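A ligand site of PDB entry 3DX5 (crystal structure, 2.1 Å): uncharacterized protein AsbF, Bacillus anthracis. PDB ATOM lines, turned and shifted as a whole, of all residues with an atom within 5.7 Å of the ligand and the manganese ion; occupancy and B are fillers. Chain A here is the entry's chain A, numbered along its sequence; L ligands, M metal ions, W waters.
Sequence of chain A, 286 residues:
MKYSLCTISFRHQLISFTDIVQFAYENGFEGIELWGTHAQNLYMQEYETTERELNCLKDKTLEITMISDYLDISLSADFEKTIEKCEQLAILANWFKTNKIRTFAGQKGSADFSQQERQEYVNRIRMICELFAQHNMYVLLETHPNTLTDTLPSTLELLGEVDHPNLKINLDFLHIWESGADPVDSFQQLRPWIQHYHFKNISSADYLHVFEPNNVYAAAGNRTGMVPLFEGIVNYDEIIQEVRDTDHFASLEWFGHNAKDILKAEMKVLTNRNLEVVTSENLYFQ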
ATOM      1  N   ILE A   8      -1.016 -14.932  18.604  1.00  0.00           N
ATOM      2  CA  ILE A   8      -0.705 -14.244  19.859  1.00  0.00           C
ATOM      3  C   ILE A   8      -1.023 -15.094  21.125  1.00  0.00           C
ATOM      4  O   ILE A   8      -0.397 -14.922  22.142  1.00  0.00           O
ATOM      5  CB  ILE A   8      -1.407 -12.844  19.943  1.00  0.00           C
ATOM      6  CG1 ILE A   8      -0.737 -11.945  21.010  1.00  0.00           C
ATOM      7  CG2 ILE A   8      -2.959 -12.977  20.111  1.00  0.00           C
ATOM      8  CD1 ILE A   8      -1.235 -10.411  20.962  1.00  0.00           C
ATOM      9  N   TRP A  35      -0.135 -12.909  14.243  1.00  0.00           N
ATOM     10  CA  TRP A  35       0.462 -11.726  14.900  1.00  0.00           C
ATOM     11  C   TRP A  35       1.592 -11.177  13.987  1.00  0.00           C
ATOM     12  O   TRP A  35       2.352 -11.967  13.412  1.00  0.00           O
ATOM     13  CB  TRP A  35       1.060 -12.206  16.215  1.00  0.00           C
ATOM     14  CG  TRP A  35       1.234 -11.167  17.278  1.00  0.00           C
ATOM     15  CD1 TRP A  35       0.623  -9.921  17.391  1.00  0.00           C
ATOM     16  CD2 TRP A  35       2.063 -11.313  18.456  1.00  0.00           C
ATOM     17  NE1 TRP A  35       1.051  -9.291  18.565  1.00  0.00           N
ATOM     18  CE2 TRP A  35       1.927 -10.130  19.218  1.00  0.00           C
ATOM     19  CE3 TRP A  35       2.902 -12.355  18.921  1.00  0.00           C
ATOM     20  CZ2 TRP A  35       2.617  -9.949  20.437  1.00  0.00           C
ATOM     21  CZ3 TRP A  35       3.587 -12.168  20.128  1.00  0.00           C
ATOM     22  CH2 TRP A  35       3.443 -10.971  20.866  1.00  0.00           C
ATOM     23  N   SER A  68      -2.138  -9.043  12.524  1.00  0.00           N
ATOM     24  CA  SER A  68      -2.496  -8.126  13.590  1.00  0.00           C
ATOM     25  C   SER A  68      -1.279  -7.458  14.206  1.00  0.00           C
ATOM     26  O   SER A  68      -0.400  -8.113  14.773  1.00  0.00           O
ATOM     27  CB  SER A  68      -3.381  -8.833  14.627  1.00  0.00           C
ATOM     28  OG  SER A  68      -4.463  -9.444  13.944  1.00  0.00           O
ATOM     29  N   TYR A  70       0.505  -3.128  15.072  1.00  0.00           N
ATOM     30  CA  TYR A  70       0.423  -1.919  15.888  1.00  0.00           C
ATOM     31  C   TYR A  70       1.090  -0.861  15.041  1.00  0.00           C
ATOM     32  O   TYR A  70       2.272  -0.970  14.737  1.00  0.00           O
ATOM     33  CB  TYR A  70       1.220  -2.086  17.226  1.00  0.00           C
ATOM     34  CG  TYR A  70       0.916  -3.404  17.957  1.00  0.00           C
ATOM     35  CD1 TYR A  70      -0.110  -3.464  18.922  1.00  0.00           C
ATOM     36  CD2 TYR A  70       1.630  -4.591  17.647  1.00  0.00           C
ATOM     37  CE1 TYR A  70      -0.415  -4.685  19.572  1.00  0.00           C
ATOM     38  CE2 TYR A  70       1.291  -5.795  18.259  1.00  0.00           C
ATOM     39  CZ  TYR A  70       0.282  -5.838  19.219  1.00  0.00           C
ATOM     40  OH  TYR A  70      -0.018  -7.041  19.842  1.00  0.00           O
ATOM     41  N   ARG A 102      -4.739  -5.377  11.225  1.00  0.00           N
ATOM     42  CA  ARG A 102      -5.358  -4.845  12.427  1.00  0.00           C
ATOM     43  C   ARG A 102      -4.420  -3.823  13.071  1.00  0.00           C
ATOM     44  O   ARG A 102      -3.218  -4.066  13.226  1.00  0.00           O
ATOM     45  CB  ARG A 102      -5.618  -6.019  13.405  1.00  0.00           C
ATOM     46  CG  ARG A 102      -6.369  -5.689  14.737  1.00  0.00           C
ATOM     47  CD  ARG A 102      -5.565  -4.841  15.797  1.00  0.00           C
ATOM     48  NE  ARG A 102      -4.215  -5.308  16.174  1.00  0.00           N
ATOM     49  CZ  ARG A 102      -3.974  -6.205  17.119  1.00  0.00           C
ATOM     50  NH1 ARG A 102      -2.710  -6.543  17.411  1.00  0.00           N
ATOM     51  NH2 ARG A 102      -5.002  -6.770  17.778  1.00  0.00           N
ATOM     52  N   PHE A 104      -4.499  -0.269  16.144  1.00  0.00           N
ATOM     53  CA  PHE A 104      -5.218   0.431  17.211  1.00  0.00           C
ATOM     54  C   PHE A 104      -5.216   1.904  16.904  1.00  0.00           C
ATOM     55  O   PHE A 104      -4.274   2.404  16.281  1.00  0.00           O
ATOM     56  CB  PHE A 104      -4.552   0.172  18.578  1.00  0.00           C
ATOM     57  CG  PHE A 104      -4.678  -1.263  19.016  1.00  0.00           C
ATOM     58  CD1 PHE A 104      -5.889  -1.749  19.504  1.00  0.00           C
ATOM     59  CD2 PHE A 104      -3.604  -2.139  18.899  1.00  0.00           C
ATOM     60  CE1 PHE A 104      -6.029  -3.071  19.890  1.00  0.00           C
ATOM     61  CE2 PHE A 104      -3.736  -3.475  19.309  1.00  0.00           C
ATOM     62  CZ  PHE A 104      -4.935  -3.936  19.781  1.00  0.00           C
ATOM     63  N   GLU A 142      -9.273  -1.941  15.909  1.00  0.00           N
ATOM     64  CA  GLU A 142      -9.849  -2.802  16.931  1.00  0.00           C
ATOM     65  C   GLU A 142     -10.539  -1.923  18.008  1.00  0.00           C
ATOM     66  O   GLU A 142     -10.012  -0.911  18.396  1.00  0.00           O
ATOM     67  CB  GLU A 142      -8.741  -3.690  17.528  1.00  0.00           C
ATOM     68  CG  GLU A 142      -9.270  -4.687  18.536  1.00  0.00           C
ATOM     69  CD  GLU A 142      -8.332  -5.840  18.729  1.00  0.00           C
ATOM     70  OE1 GLU A 142      -7.678  -6.279  17.759  1.00  0.00           O
ATOM     71  OE2 GLU A 142      -8.256  -6.317  19.866  1.00  0.00           O
ATOM     72  N   HIS A 144     -11.136  -0.936  21.508  1.00  0.00           N
ATOM     73  CA  HIS A 144     -10.248  -1.091  22.661  1.00  0.00           C
ATOM     74  C   HIS A 144     -10.329   0.071  23.652  1.00  0.00           C
ATOM     75  O   HIS A 144     -10.386   1.222  23.209  1.00  0.00           O
ATOM     76  CB  HIS A 144      -8.806  -1.140  22.189  1.00  0.00           C
ATOM     77  CG  HIS A 144      -8.148  -2.435  22.504  1.00  0.00           C
ATOM     78  ND1 HIS A 144      -7.005  -2.526  23.266  1.00  0.00           N
ATOM     79  CD2 HIS A 144      -8.543  -3.706  22.233  1.00  0.00           C
ATOM     80  CE1 HIS A 144      -6.678  -3.797  23.373  1.00  0.00           C
ATOM     81  NE2 HIS A 144      -7.601  -4.532  22.770  1.00  0.00           N
ATOM     82  N   ASN A 170     -12.372  -4.230  13.503  1.00  0.00           N
ATOM     83  CA  ASN A 170     -12.294  -5.513  14.169  1.00  0.00           C
ATOM     84  C   ASN A 170     -13.079  -5.376  15.476  1.00  0.00           C
ATOM     85  O   ASN A 170     -12.630  -4.683  16.417  1.00  0.00           O
ATOM     86  CB  ASN A 170     -10.833  -5.900  14.510  1.00  0.00           C
ATOM     87  CG  ASN A 170     -10.764  -7.277  15.171  1.00  0.00           C
ATOM     88  OD1 ASN A 170     -11.609  -8.129  14.922  1.00  0.00           O
ATOM     89  ND2 ASN A 170      -9.810  -7.464  16.048  1.00  0.00           N
ATOM     90  N   ASP A 172     -14.279  -6.232  18.930  1.00  0.00           N
ATOM     91  CA  ASP A 172     -13.844  -7.052  20.085  1.00  0.00           C
ATOM     92  C   ASP A 172     -14.961  -6.870  21.128  1.00  0.00           C
ATOM     93  O   ASP A 172     -15.036  -5.835  21.805  1.00  0.00           O
ATOM     94  CB  ASP A 172     -12.462  -6.565  20.546  1.00  0.00           C
ATOM     95  CG  ASP A 172     -11.859  -7.418  21.657  1.00  0.00           C
ATOM     96  OD1 ASP A 172     -12.579  -7.855  22.580  1.00  0.00           O
ATOM     97  OD2 ASP A 172     -10.632  -7.605  21.631  1.00  0.00           O
ATOM     98  N   HIS A 175     -14.399  -5.830  24.889  1.00  0.00           N
ATOM     99  CA  HIS A 175     -14.087  -4.448  25.106  1.00  0.00           C
ATOM    100  C   HIS A 175     -15.255  -3.525  24.861  1.00  0.00           C
ATOM    101  O   HIS A 175     -15.362  -2.482  25.494  1.00  0.00           O
ATOM    102  CB  HIS A 175     -12.847  -4.023  24.297  1.00  0.00           C
ATOM    103  CG  HIS A 175     -11.607  -4.699  24.785  1.00  0.00           C
ATOM    104  ND1 HIS A 175     -11.238  -4.684  26.110  1.00  0.00           N
ATOM    105  CD2 HIS A 175     -10.704  -5.478  24.142  1.00  0.00           C
ATOM    106  CE1 HIS A 175     -10.120  -5.386  26.249  1.00  0.00           C
ATOM    107  NE2 HIS A 175      -9.774  -5.871  25.075  1.00  0.00           N
ATOM    108  N   HIS A 198     -13.200 -10.403  17.453  1.00  0.00           N
ATOM    109  CA  HIS A 198     -12.458 -11.062  18.545  1.00  0.00           C
ATOM    110  C   HIS A 198     -13.471 -11.489  19.568  1.00  0.00           C
ATOM    111  O   HIS A 198     -14.311 -10.684  19.976  1.00  0.00           O
ATOM    112  CB  HIS A 198     -11.460 -10.080  19.197  1.00  0.00           C
ATOM    113  CG  HIS A 198     -10.158  -9.977  18.470  1.00  0.00           C
ATOM    114  ND1 HIS A 198      -9.100  -9.205  18.921  1.00  0.00           N
ATOM    115  CD2 HIS A 198      -9.735 -10.570  17.321  1.00  0.00           C
ATOM    116  CE1 HIS A 198      -8.071  -9.345  18.090  1.00  0.00           C
ATOM    117  NE2 HIS A 198      -8.434 -10.164  17.111  1.00  0.00           N
ATOM    118  N   LYS A 200     -13.598 -12.980  23.406  1.00  0.00           N
ATOM    119  CA  LYS A 200     -12.988 -13.464  24.655  1.00  0.00           C
ATOM    120  C   LYS A 200     -13.948 -13.070  25.774  1.00  0.00           C
ATOM    121  O   LYS A 200     -14.869 -12.276  25.550  1.00  0.00           O
ATOM    122  CB  LYS A 200     -11.549 -12.903  24.858  1.00  0.00           C
ATOM    123  CG  LYS A 200     -11.408 -11.345  24.885  1.00  0.00           C
ATOM    124  CD  LYS A 200      -9.948 -10.954  25.200  1.00  0.00           C
ATOM    125  CE  LYS A 200      -9.748  -9.419  25.303  1.00  0.00           C
ATOM    126  NZ  LYS A 200     -10.014  -8.723  23.998  1.00  0.00           N
ATOM    127  N   PHE A 211      -6.711  -7.572  30.981  1.00  0.00           N
ATOM    128  CA  PHE A 211      -6.523  -7.309  29.562  1.00  0.00           C
ATOM    129  C   PHE A 211      -5.691  -6.090  29.206  1.00  0.00           C
ATOM    130  O   PHE A 211      -5.493  -5.815  28.024  1.00  0.00           O
ATOM    131  CB  PHE A 211      -7.847  -7.271  28.826  1.00  0.00           C
ATOM    132  CG  PHE A 211      -8.594  -8.563  28.901  1.00  0.00           C
ATOM    133  CD1 PHE A 211      -7.979  -9.774  28.537  1.00  0.00           C
ATOM    134  CD2 PHE A 211      -9.895  -8.580  29.372  1.00  0.00           C
ATOM    135  CE1 PHE A 211      -8.683 -10.988  28.615  1.00  0.00           C
ATOM    136  CE2 PHE A 211     -10.603  -9.788  29.438  1.00  0.00           C
ATOM    137  CZ  PHE A 211      -9.994 -10.983  29.067  1.00  0.00           C
ATOM    138  N   GLU A 212      -5.192  -5.364  30.189  1.00  0.00           N
ATOM    139  CA  GLU A 212      -4.310  -4.279  29.836  1.00  0.00           C
ATOM    140  C   GLU A 212      -3.088  -4.862  29.094  1.00  0.00           C
ATOM    141  O   GLU A 212      -2.528  -5.871  29.531  1.00  0.00           O
ATOM    142  CB  GLU A 212      -3.864  -3.516  31.092  1.00  0.00           C
ATOM    143  CG  GLU A 212      -5.023  -2.690  31.691  1.00  0.00           C
ATOM    144  CD  GLU A 212      -4.663  -2.058  33.033  1.00  0.00           C
ATOM    145  OE1 GLU A 212      -3.453  -2.078  33.373  1.00  0.00           O
ATOM    146  OE2 GLU A 212      -5.571  -1.560  33.745  1.00  0.00           O
ATOM    147  N   PRO A 213      -2.684  -4.227  27.976  1.00  0.00           N
ATOM    148  CA  PRO A 213      -1.636  -4.764  27.101  1.00  0.00           C
ATOM    149  C   PRO A 213      -0.360  -5.129  27.871  1.00  0.00           C
ATOM    150  O   PRO A 213       0.182  -6.206  27.672  1.00  0.00           O
ATOM    151  CB  PRO A 213      -1.416  -3.642  26.058  1.00  0.00           C
ATOM    152  CG  PRO A 213      -2.858  -3.095  25.890  1.00  0.00           C
ATOM    153  CD  PRO A 213      -3.375  -3.049  27.357  1.00  0.00           C
ATOM    154  N   VAL A 216      -0.982  -8.407  29.564  1.00  0.00           N
ATOM    155  CA  VAL A 216      -1.097  -9.446  28.539  1.00  0.00           C
ATOM    156  C   VAL A 216       0.280  -9.857  27.995  1.00  0.00           C
ATOM    157  O   VAL A 216       0.549 -11.066  27.845  1.00  0.00           O
ATOM    158  CB  VAL A 216      -2.053  -9.040  27.401  1.00  0.00           C
ATOM    159  CG1 VAL A 216      -1.918 -10.016  26.163  1.00  0.00           C
ATOM    160  CG2 VAL A 216      -3.510  -9.029  27.891  1.00  0.00           C
ATOM    161  N   TYR A 217       1.164  -8.878  27.719  1.00  0.00           N
ATOM    162  CA  TYR A 217       2.452  -9.203  27.085  1.00  0.00           C
ATOM    163  C   TYR A 217       3.495  -9.799  28.038  1.00  0.00           C
ATOM    164  O   TYR A 217       4.404 -10.495  27.572  1.00  0.00           O
ATOM    165  CB  TYR A 217       3.092  -8.001  26.342  1.00  0.00           C
ATOM    166  CG  TYR A 217       2.124  -7.302  25.401  1.00  0.00           C
ATOM    167  CD1 TYR A 217       1.183  -8.019  24.645  1.00  0.00           C
ATOM    168  CD2 TYR A 217       2.179  -5.904  25.254  1.00  0.00           C
ATOM    169  CE1 TYR A 217       0.271  -7.356  23.783  1.00  0.00           C
ATOM    170  CE2 TYR A 217       1.304  -5.243  24.387  1.00  0.00           C
ATOM    171  CZ  TYR A 217       0.348  -5.957  23.679  1.00  0.00           C
ATOM    172  OH  TYR A 217      -0.502  -5.238  22.843  1.00  0.00           O
ATOM    173  N   GLU A 253      -9.763 -15.184  20.952  1.00  0.00           N
ATOM    174  CA  GLU A 253      -8.600 -14.444  21.432  1.00  0.00           C
ATOM    175  C   GLU A 253      -8.280 -14.812  22.862  1.00  0.00           C
ATOM    176  O   GLU A 253      -8.577 -14.043  23.801  1.00  0.00           O
ATOM    177  CB  GLU A 253      -8.881 -12.944  21.357  1.00  0.00           C
ATOM    178  CG  GLU A 253      -7.610 -12.081  21.438  1.00  0.00           C
ATOM    179  CD  GLU A 253      -7.917 -10.590  21.367  1.00  0.00           C
ATOM    180  OE1 GLU A 253      -9.008 -10.198  21.841  1.00  0.00           O
ATOM    181  OE2 GLU A 253      -7.073  -9.822  20.839  1.00  0.00           O
ATOM    182  N   PHE A 255      -5.836 -15.242  25.955  1.00  0.00           N
ATOM    183  CA  PHE A 255      -4.583 -14.720  26.472  1.00  0.00           C
ATOM    184  C   PHE A 255      -4.127 -15.508  27.719  1.00  0.00           C
ATOM    185  O   PHE A 255      -3.115 -15.179  28.316  1.00  0.00           O
ATOM    186  CB  PHE A 255      -4.752 -13.252  26.836  1.00  0.00           C
ATOM    187  CG  PHE A 255      -4.883 -12.340  25.650  1.00  0.00           C
ATOM    188  CD1 PHE A 255      -3.990 -12.451  24.572  1.00  0.00           C
ATOM    189  CD2 PHE A 255      -5.860 -11.353  25.617  1.00  0.00           C
ATOM    190  CE1 PHE A 255      -4.040 -11.603  23.517  1.00  0.00           C
ATOM    191  CE2 PHE A 255      -5.933 -10.476  24.527  1.00  0.00           C
ATOM    192  CZ  PHE A 255      -5.030 -10.608  23.467  1.00  0.00           C
HETATM  193  C1  LIG L   1      -4.176  -7.101  22.372  1.00  0.00           C
HETATM  194  C2  LIG L   1      -5.509  -7.298  22.017  1.00  0.00           C
HETATM  195  C3  LIG L   1      -6.522  -7.251  22.985  1.00  0.00           C
HETATM  196  O1  LIG L   1      -7.852  -7.437  22.710  1.00  0.00           O
HETATM  197  C4  LIG L   1      -6.138  -6.960  24.369  1.00  0.00           C
HETATM  198  O2  LIG L   1      -7.140  -6.918  25.271  1.00  0.00           O
HETATM  199  C5  LIG L   1      -4.802  -6.738  24.704  1.00  0.00           C
HETATM  200  C6  LIG L   1      -3.839  -6.817  23.694  1.00  0.00           C
HETATM  201  C7  LIG L   1      -3.106  -7.176  21.294  1.00  0.00           C
HETATM  202  O3  LIG L   1      -1.913  -6.970  21.509  1.00  0.00           O
HETATM  203  O4  LIG L   1      -3.455  -7.497  20.048  1.00  0.00           O
HETATM  204 MN    MN M   1      -8.695  -8.086  20.863  1.00  0.00          MN
HETATM  205  O   HOH W   1      -6.940  -3.811  26.442  1.00  0.00           O
HETATM  206  O   HOH W   2      -4.838  -9.933  19.486  1.00  0.00           O
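OH of Tyr 70 is in hydrogen-bond range of O3 of the ligand (2.5 Å). The side-chain hydroxyl (OH) of Tyr 217 lies within hydrogen-bond range of an oxygen (O3) of the ligand (2.6 Å). The side-chain amino group (NZ) of Lys 200 lies close to an oxygen (O1) of the ligand, 2.8 Å away. NE2 of His 175 sits at hydrogen-bond distance from O2 of the ligand. The guanidinium group of Arg 102 is in salt-bridge range of an oxygen (O4) of the ligand (2.8 Å). A ring nitrogen (NE2) of His 144 sits close to an oxygen (O2) of the ligand, at 3.5 Å. The backbone carbonyl oxygen (O) of Phe 211 lies within hydrogen-bond range of an oxygen (O2) of the ligand.
The side-chain carboxylate of Glu 142 lies within salt-bridge range of the guanidinium group of Arg 102, at 2.7 Å. OE2 of Glu 142 lies close to NE2 of His 144, 3.5 Å away. OE1 of Glu 142 sits at hydrogen-bond distance from ND2 of Asn 170 (3.0 Å). The side-chain amino group (NZ) of Lys 200 is in salt-bridge range of the side-chain carboxylate (OD1) of Asp 172 (3.1 Å). A ring nitrogen (NE2) of His 198 lies within hydrogen-bond range of the side-chain amide nitrogen (ND2) of Asn 170 (3.2 Å). The side-chain carboxylate (OE1) of Glu 253 sits close to the side-chain amino group (NZ) of Lys 200. The side-chain hydroxyl (OH) of Tyr 70 lies within hydrogen-bond range of the indole nitrogen (NE1) of Trp 35. A ring nitrogen (NE2) of His 175 sits at hydrogen-bond distance from a ring nitrogen (NE2) of His 144, 3.4 Å away.
Merely in contact with the ligand: Phe 255, Ile 8 and Phe 104. Hydrophobic or aromatic side chains within 4 Å of the ligand: Ile 8, Tyr 70, Phe 104, His 144, His 175, Phe 211, Tyr 217 and Phe 255. Along chain A the residues within 4 Å of the ligand span positions 8 to 255. The nearest printed residue that does not touch the ligand is Val 216 (4.1 Å).
Residues that only touch the manganese ion: Lys 200 (3.5 Å). Five residues have an atom within 4 Å of the manganese ion: Glu 142, Asp 172, His 198, Lys 200 and Glu 253.
The manganese ion is bound by OE2 of Glu 142 (2.1 Å), O1 of the ligand (2.1 Å), OD2 of Asp 172 (2.1 Å), ND1 of His 198 (2.3 Å), OE1 of Glu 253 (2.3 Å) and OE2 of Glu 253 (2.4 Å). The manganese ion has six donor atoms within binding distance.
Water W1 lies within hydrogen-bond range of the backbone carbonyl oxygen (O) of Phe 211, an oxygen (O2) of the ligand and a ring nitrogen (ND1) of His 144.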
